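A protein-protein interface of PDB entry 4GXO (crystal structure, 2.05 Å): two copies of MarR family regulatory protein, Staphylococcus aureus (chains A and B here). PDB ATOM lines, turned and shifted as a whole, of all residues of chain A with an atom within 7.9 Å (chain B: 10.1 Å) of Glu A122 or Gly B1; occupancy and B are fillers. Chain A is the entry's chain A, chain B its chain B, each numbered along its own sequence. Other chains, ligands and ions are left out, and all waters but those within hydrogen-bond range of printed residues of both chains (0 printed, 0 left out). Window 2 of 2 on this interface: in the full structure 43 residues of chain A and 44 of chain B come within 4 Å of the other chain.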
ATOM      1  N   ASN A 119     -13.858 -25.154  26.221  1.00  0.00           N
ATOM      2  CA  ASN A 119     -14.552 -24.485  25.117  1.00  0.00           C
ATOM      3  C   ASN A 119     -13.845 -23.216  24.666  1.00  0.00           C
ATOM      4  O   ASN A 119     -14.418 -22.125  24.664  1.00  0.00           O
ATOM      5  CB  ASN A 119     -16.006 -24.181  25.488  1.00  0.00           C
ATOM      6  CG  ASN A 119     -16.804 -23.616  24.321  1.00  0.00           C
ATOM      7  OD1 ASN A 119     -16.619 -24.015  23.166  1.00  0.00           O
ATOM      8  ND2 ASN A 119     -17.694 -22.676  24.617  1.00  0.00           N
ATOM      9  N   ILE A 120     -12.585 -23.370  24.292  1.00  0.00           N
ATOM     10  CA  ILE A 120     -11.850 -22.280  23.683  1.00  0.00           C
ATOM     11  C   ILE A 120     -11.692 -22.561  22.185  1.00  0.00           C
ATOM     12  O   ILE A 120     -11.734 -23.707  21.746  1.00  0.00           O
ATOM     13  CB  ILE A 120     -10.496 -22.011  24.406  1.00  0.00           C
ATOM     14  CG1 ILE A 120      -9.624 -23.270  24.494  1.00  0.00           C
ATOM     15  CG2 ILE A 120     -10.743 -21.484  25.813  1.00  0.00           C
ATOM     16  CD1 ILE A 120      -8.321 -23.071  25.251  1.00  0.00           C
ATOM     17  N   SER A 121     -11.533 -21.497  21.408  1.00  0.00           N
ATOM     18  CA  SER A 121     -11.345 -21.608  19.963  1.00  0.00           C
ATOM     19  C   SER A 121      -9.959 -22.154  19.628  1.00  0.00           C
ATOM     20  O   SER A 121      -9.046 -22.109  20.463  1.00  0.00           O
ATOM     21  CB  SER A 121     -11.491 -20.236  19.329  1.00  0.00           C
ATOM     22  OG  SER A 121     -10.416 -19.392  19.734  1.00  0.00           O
ATOM     23  N   GLU A 122      -9.794 -22.651  18.408  1.00  0.00           N
ATOM     24  CA  GLU A 122      -8.477 -23.105  17.953  1.00  0.00           C
ATOM     25  C   GLU A 122      -7.420 -21.986  17.971  1.00  0.00           C
ATOM     26  O   GLU A 122      -6.244 -22.256  18.215  1.00  0.00           O
ATOM     27  CB  GLU A 122      -8.555 -23.742  16.564  1.00  0.00           C
ATOM     28  CG  GLU A 122      -9.047 -25.181  16.613  1.00  0.00           C
ATOM     29  CD  GLU A 122      -9.155 -25.821  15.237  1.00  0.00           C
ATOM     30  OE1 GLU A 122      -8.350 -25.473  14.340  1.00  0.00           O
ATOM     31  OE2 GLU A 122     -10.048 -26.672  15.060  1.00  0.00           O
ATOM     32  N   ARG A 123      -7.852 -20.752  17.727  1.00  0.00           N
ATOM     33  CA  ARG A 123      -6.973 -19.593  17.771  1.00  0.00           C
ATOM     34  C   ARG A 123      -6.498 -19.327  19.204  1.00  0.00           C
ATOM     35  O   ARG A 123      -5.299 -19.109  19.437  1.00  0.00           O
ATOM     36  CB  ARG A 123      -7.699 -18.369  17.216  1.00  0.00           C
ATOM     37  CG  ARG A 123      -6.798 -17.261  16.692  1.00  0.00           C
ATOM     38  CD  ARG A 123      -6.318 -16.318  17.778  1.00  0.00           C
ATOM     39  NE  ARG A 123      -6.021 -14.983  17.241  1.00  0.00           N
ATOM     40  CZ  ARG A 123      -4.837 -14.570  16.774  1.00  0.00           C
ATOM     41  NH1 ARG A 123      -3.768 -15.373  16.754  1.00  0.00           N
ATOM     42  NH2 ARG A 123      -4.719 -13.327  16.318  1.00  0.00           N
ATOM     43  N   GLU A 124      -7.449 -19.349  20.142  1.00  0.00           N
ATOM     44  CA  GLU A 124      -7.179 -19.202  21.577  1.00  0.00           C
ATOM     45  C   GLU A 124      -6.266 -20.314  22.077  1.00  0.00           C
ATOM     46  O   GLU A 124      -5.285 -20.039  22.755  1.00  0.00           O
ATOM     47  CB  GLU A 124      -8.484 -19.167  22.388  1.00  0.00           C
ATOM     48  CG  GLU A 124      -9.225 -17.827  22.290  1.00  0.00           C
ATOM     49  CD  GLU A 124     -10.710 -17.864  22.695  1.00  0.00           C
ATOM     50  OE1 GLU A 124     -11.274 -18.935  23.035  1.00  0.00           O
ATOM     51  OE2 GLU A 124     -11.335 -16.782  22.669  1.00  0.00           O
ATOM     52  N   ALA A 125      -6.583 -21.559  21.734  1.00  0.00           N
ATOM     53  CA  ALA A 125      -5.728 -22.697  22.083  1.00  0.00           C
ATOM     54  C   ALA A 125      -4.313 -22.539  21.509  1.00  0.00           C
ATOM     55  O   ALA A 125      -3.329 -22.725  22.212  1.00  0.00           O
ATOM     56  CB  ALA A 125      -6.350 -23.988  21.594  1.00  0.00           C
ATOM     57  N   SER A 126      -4.222 -22.162  20.236  1.00  0.00           N
ATOM     58  CA  SER A 126      -2.934 -21.978  19.586  1.00  0.00           C
ATOM     59  C   SER A 126      -2.160 -20.844  20.272  1.00  0.00           C
ATOM     60  O   SER A 126      -0.936 -20.949  20.429  1.00  0.00           O
ATOM     61  CB  SER A 126      -3.102 -21.711  18.083  1.00  0.00           C
ATOM     62  OG  SER A 126      -1.845 -21.615  17.431  1.00  0.00           O
ATOM     63  N   ASP A 127      -2.865 -19.802  20.713  1.00  0.00           N
ATOM     64  CA  ASP A 127      -2.209 -18.668  21.366  1.00  0.00           C
ATOM     65  C   ASP A 127      -1.730 -19.051  22.759  1.00  0.00           C
ATOM     66  O   ASP A 127      -0.633 -18.666  23.141  1.00  0.00           O
ATOM     67  CB  ASP A 127      -3.103 -17.428  21.438  1.00  0.00           C
ATOM     68  CG  ASP A 127      -3.228 -16.717  20.096  1.00  0.00           C
ATOM     69  OD1 ASP A 127      -2.519 -17.100  19.132  1.00  0.00           O
ATOM     70  OD2 ASP A 127      -4.044 -15.773  20.002  1.00  0.00           O
ATOM     71  N   ILE A 128      -2.537 -19.815  23.501  1.00  0.00           N
ATOM     72  CA  ILE A 128      -2.104 -20.323  24.815  1.00  0.00           C
ATOM     73  C   ILE A 128      -0.825 -21.142  24.626  1.00  0.00           C
ATOM     74  O   ILE A 128       0.178 -20.941  25.325  1.00  0.00           O
ATOM     75  CB  ILE A 128      -3.209 -21.163  25.484  1.00  0.00           C
ATOM     76  CG1 ILE A 128      -4.359 -20.264  25.923  1.00  0.00           C
ATOM     77  CG2 ILE A 128      -2.686 -21.923  26.696  1.00  0.00           C
ATOM     78  CD1 ILE A 128      -5.561 -21.008  26.485  1.00  0.00           C
ATOM     79  N   ILE A 129      -0.872 -22.054  23.658  1.00  0.00           N
ATOM     80  CA  ILE A 129       0.243 -22.919  23.325  1.00  0.00           C
ATOM     81  C   ILE A 129       1.515 -22.141  23.013  1.00  0.00           C
ATOM     82  O   ILE A 129       2.558 -22.412  23.601  1.00  0.00           O
ATOM     83  CB  ILE A 129      -0.116 -23.851  22.163  1.00  0.00           C
ATOM     84  CG1 ILE A 129      -1.100 -24.918  22.659  1.00  0.00           C
ATOM     85  CG2 ILE A 129       1.122 -24.538  21.595  1.00  0.00           C
ATOM     86  CD1 ILE A 129      -1.883 -25.557  21.549  1.00  0.00           C
ATOM     87  N   GLY B   1      -3.881 -28.752  14.862  1.00  0.00           N
ATOM     88  CA  GLY B   1      -5.135 -28.359  14.154  1.00  0.00           C
ATOM     89  C   GLY B   1      -6.320 -29.232  14.518  1.00  0.00           C
ATOM     90  O   GLY B   1      -7.395 -28.721  14.861  1.00  0.00           O
ATOM     91  N   SER B   2      -6.126 -30.549  14.431  1.00  0.00           N
ATOM     92  CA  SER B   2      -7.030 -31.488  15.066  1.00  0.00           C
ATOM     93  C   SER B   2      -6.986 -31.142  16.535  1.00  0.00           C
ATOM     94  O   SER B   2      -5.974 -30.599  17.043  1.00  0.00           O
ATOM     95  CB  SER B   2      -6.587 -32.951  14.866  1.00  0.00           C
ATOM     96  OG  SER B   2      -5.528 -33.332  15.753  1.00  0.00           O
ATOM     97  N   HIS B   3      -8.065 -31.450  17.236  1.00  0.00           N
ATOM     98  CA  HIS B   3      -8.109 -31.120  18.638  1.00  0.00           C
ATOM     99  C   HIS B   3      -7.241 -32.089  19.430  1.00  0.00           C
ATOM    100  O   HIS B   3      -6.842 -31.779  20.551  1.00  0.00           O
ATOM    101  CB  HIS B   3      -9.550 -31.052  19.114  1.00  0.00           C
ATOM    102  CG  HIS B   3     -10.287 -29.859  18.586  1.00  0.00           C
ATOM    103  ND1 HIS B   3     -11.531 -29.484  19.046  1.00  0.00           N
ATOM    104  CD2 HIS B   3      -9.933 -28.933  17.663  1.00  0.00           C
ATOM    105  CE1 HIS B   3     -11.917 -28.386  18.421  1.00  0.00           C
ATOM    106  NE2 HIS B   3     -10.967 -28.031  17.575  1.00  0.00           N
ATOM    107  N   MET B   4      -6.908 -33.234  18.829  1.00  0.00           N
ATOM    108  CA  MET B   4      -6.021 -34.199  19.469  1.00  0.00           C
ATOM    109  C   MET B   4      -4.632 -33.603  19.640  1.00  0.00           C
ATOM    110  O   MET B   4      -4.069 -33.658  20.742  1.00  0.00           O
ATOM    111  CB  MET B   4      -5.948 -35.519  18.687  1.00  0.00           C
ATOM    112  CG  MET B   4      -4.989 -36.551  19.283  1.00  0.00           C
ATOM    113  SD  MET B   4      -5.446 -37.113  20.942  1.00  0.00           S
ATOM    114  CE  MET B   4      -6.854 -38.145  20.536  1.00  0.00           C
ATOM    115  N   TYR B   5      -4.089 -33.012  18.575  1.00  0.00           N
ATOM    116  CA  TYR B   5      -2.752 -32.434  18.653  1.00  0.00           C
ATOM    117  C   TYR B   5      -2.683 -31.227  19.584  1.00  0.00           C
ATOM    118  O   TYR B   5      -1.757 -31.135  20.400  1.00  0.00           O
ATOM    119  CB  TYR B   5      -2.185 -32.063  17.282  1.00  0.00           C
ATOM    120  CG  TYR B   5      -0.820 -31.415  17.372  1.00  0.00           C
ATOM    121  CD1 TYR B   5       0.336 -32.183  17.523  1.00  0.00           C
ATOM    122  CD2 TYR B   5      -0.679 -30.031  17.336  1.00  0.00           C
ATOM    123  CE1 TYR B   5       1.585 -31.592  17.615  1.00  0.00           C
ATOM    124  CE2 TYR B   5       0.571 -29.430  17.432  1.00  0.00           C
ATOM    125  CZ  TYR B   5       1.700 -30.220  17.569  1.00  0.00           C
ATOM    126  OH  TYR B   5       2.947 -29.627  17.655  1.00  0.00           O
ATOM    127  N   LEU B   6      -3.638 -30.305  19.461  1.00  0.00           N
ATOM    128  CA  LEU B   6      -3.663 -29.146  20.325  1.00  0.00           C
ATOM    129  C   LEU B   6      -3.775 -29.587  21.802  1.00  0.00           C
ATOM    130  O   LEU B   6      -3.082 -29.046  22.663  1.00  0.00           O
ATOM    131  CB  LEU B   6      -4.815 -28.191  19.962  1.00  0.00           C
ATOM    132  CG  LEU B   6      -4.799 -27.493  18.592  1.00  0.00           C
ATOM    133  CD1 LEU B   6      -6.103 -26.724  18.365  1.00  0.00           C
ATOM    134  CD2 LEU B   6      -3.606 -26.560  18.426  1.00  0.00           C
ATOM    135  N   SER B   7      -4.627 -30.574  22.075  1.00  0.00           N
ATOM    136  CA  SER B   7      -4.839 -31.047  23.445  1.00  0.00           C
ATOM    137  C   SER B   7      -3.594 -31.675  24.041  1.00  0.00           C
ATOM    138  O   SER B   7      -3.352 -31.521  25.236  1.00  0.00           O
ATOM    139  CB  SER B   7      -6.026 -32.013  23.551  1.00  0.00           C
ATOM    140  OG  SER B   7      -5.641 -33.358  23.308  1.00  0.00           O
ATOM    141  N   LYS B   8      -2.802 -32.371  23.225  1.00  0.00           N
ATOM    142  CA  LYS B   8      -1.543 -32.947  23.705  1.00  0.00           C
ATOM    143  C   LYS B   8      -0.512 -31.859  24.023  1.00  0.00           C
ATOM    144  O   LYS B   8       0.288 -32.027  24.948  1.00  0.00           O
ATOM    145  CB  LYS B   8      -0.945 -33.929  22.694  1.00  0.00           C
ATOM    146  CG  LYS B   8      -1.768 -35.191  22.457  1.00  0.00           C
ATOM    147  CD  LYS B   8      -1.838 -36.073  23.698  1.00  0.00           C
ATOM    148  CE  LYS B   8      -2.667 -37.304  23.400  1.00  0.00           C
ATOM    149  NZ  LYS B   8      -3.600 -37.637  24.497  1.00  0.00           N
ATOM    150  N   GLN B   9      -0.528 -30.770  23.245  1.00  0.00           N
ATOM    151  CA  GLN B   9       0.362 -29.622  23.470  1.00  0.00           C
ATOM    152  C   GLN B   9      -0.037 -28.845  24.712  1.00  0.00           C
ATOM    153  O   GLN B   9       0.809 -28.473  25.533  1.00  0.00           O
ATOM    154  CB  GLN B   9       0.351 -28.685  22.265  1.00  0.00           C
ATOM    155  CG  GLN B   9       1.045 -29.248  21.036  1.00  0.00           C
ATOM    156  CD  GLN B   9       2.501 -29.583  21.291  1.00  0.00           C
ATOM    157  OE1 GLN B   9       2.950 -30.676  20.984  1.00  0.00           O
ATOM    158  NE2 GLN B   9       3.240 -28.651  21.885  1.00  0.00           N
ATOM    159  N   LEU B  10      -1.332 -28.576  24.824  1.00  0.00           N
ATOM    160  CA  LEU B  10      -1.882 -27.977  26.031  1.00  0.00           C
ATOM    161  C   LEU B  10      -1.569 -28.839  27.264  1.00  0.00           C
ATOM    162  O   LEU B  10      -1.131 -28.310  28.280  1.00  0.00           O
ATOM    163  CB  LEU B  10      -3.399 -27.754  25.888  1.00  0.00           C
ATOM    164  CG  LEU B  10      -3.856 -26.651  24.918  1.00  0.00           C
ATOM    165  CD1 LEU B  10      -5.338 -26.783  24.643  1.00  0.00           C
ATOM    166  CD2 LEU B  10      -3.550 -25.280  25.479  1.00  0.00           C
ATOM    167  N   ASN B 134      -9.320 -16.215  30.684  1.00  0.00           N
ATOM    168  CA  ASN B 134     -10.344 -16.697  29.770  1.00  0.00           C
ATOM    169  C   ASN B 134     -10.458 -18.221  29.826  1.00  0.00           C
ATOM    170  O   ASN B 134     -11.548 -18.785  29.694  1.00  0.00           O
ATOM    171  CB  ASN B 134     -10.019 -16.271  28.345  1.00  0.00           C
ATOM    172  CG  ASN B 134     -11.029 -16.789  27.355  1.00  0.00           C
ATOM    173  OD1 ASN B 134     -12.158 -16.306  27.318  1.00  0.00           O
ATOM    174  ND2 ASN B 134     -10.643 -17.788  26.564  1.00  0.00           N
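Of the 11 printed residues of chain B, 6 touch a printed residue of chain A. Printed residues of chain B that touch a printed residue of chain A: Gly B1, His B3, Leu B6, Gln B9, Leu B10 and Asn B134. Printed residues of chain A that touch a printed residue of chain B: Ile A120, Glu A122, Glu A124, Ile A128 and Ile A129. Hydrophobic or aromatic side chains of chain A within 4 Å of the printed part of chain B: Ile A120, Ile A128 and Ile A129. Among the printed residues, 9 pairs touch across the chains. Among the printed residues, no Asp or Glu carboxylate lies within 4 Å of a Lys or Arg side-chain nitrogen of the other chain.
OE2 of Glu A122 sits at hydrogen-bond distance from NE2 of His B3, 3.0 Å away. The backbone carbonyl oxygen (O) of Gly B1 lies close to the side-chain carboxylate (OE2) of Glu A122 (3.4 Å).
Ile A120 touches Asn B134. CG of Glu A122 touches CD1 of Leu B6 (3.8 Å). Asn B134 touches Glu A124 (ND2 to OE1, 3.8 Å). CD2 of Leu B10 touches CG2 of Ile A128, at 3.7 Å. Leu B6 touches Ile A129 (CD2 to CD1, 3.7 Å). CD1 of Ile A129 touches CB of Gln B9 (3.9 Å). Ile A129 touches Leu B10.
The backbone NH (N) of Glu A124 sits at hydrogen-bond distance from the side-chain hydroxyl (OG) of Ser A121, at 3.0 Å. The side-chain hydroxyl (OG) of Ser B7 lies close to the backbone carbonyl oxygen (O) of His B3. OH of Tyr B5 sits at hydrogen-bond distance from OE1 of Gln B9, 3.5 Å away.
No position is printed for both chains. Of the 9 pairs that touch across the chains among the printed residues, none has its exchanged pair printed and touching as well.
Glu A122 touches just these residues of chain B: Gly B1 (3.4 Å), His B3 (3.0 Å) and Leu B6 (3.8 Å). No residue of chain B comes within 4 Å of Ser A121. No residue of chain B comes within 4 Å of Ala A125. No residue of chain B comes within 4 Å of Ser A126. Of the printed residues of chain B, Ile A129 touches Leu B6, Gln B9 and Leu B10. Of the printed residues of chain B, Ile A128 touches Leu B10 (3.7 Å). Of the printed residues of chain B, Ile A120 touches Asn B134 (3.8 Å). Of the printed residues of chain B, Glu A124 touches Asn B134. Of the printed residues of chain A, Leu B6 touches Glu A122 and Ile A129. Lys B8 touches none of the printed residues of chain A. Ser B7 touches none of the printed residues of chain A. The nearest residue of chain B that does not touch Glu A122 is Ser B2 (5.5 Å).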
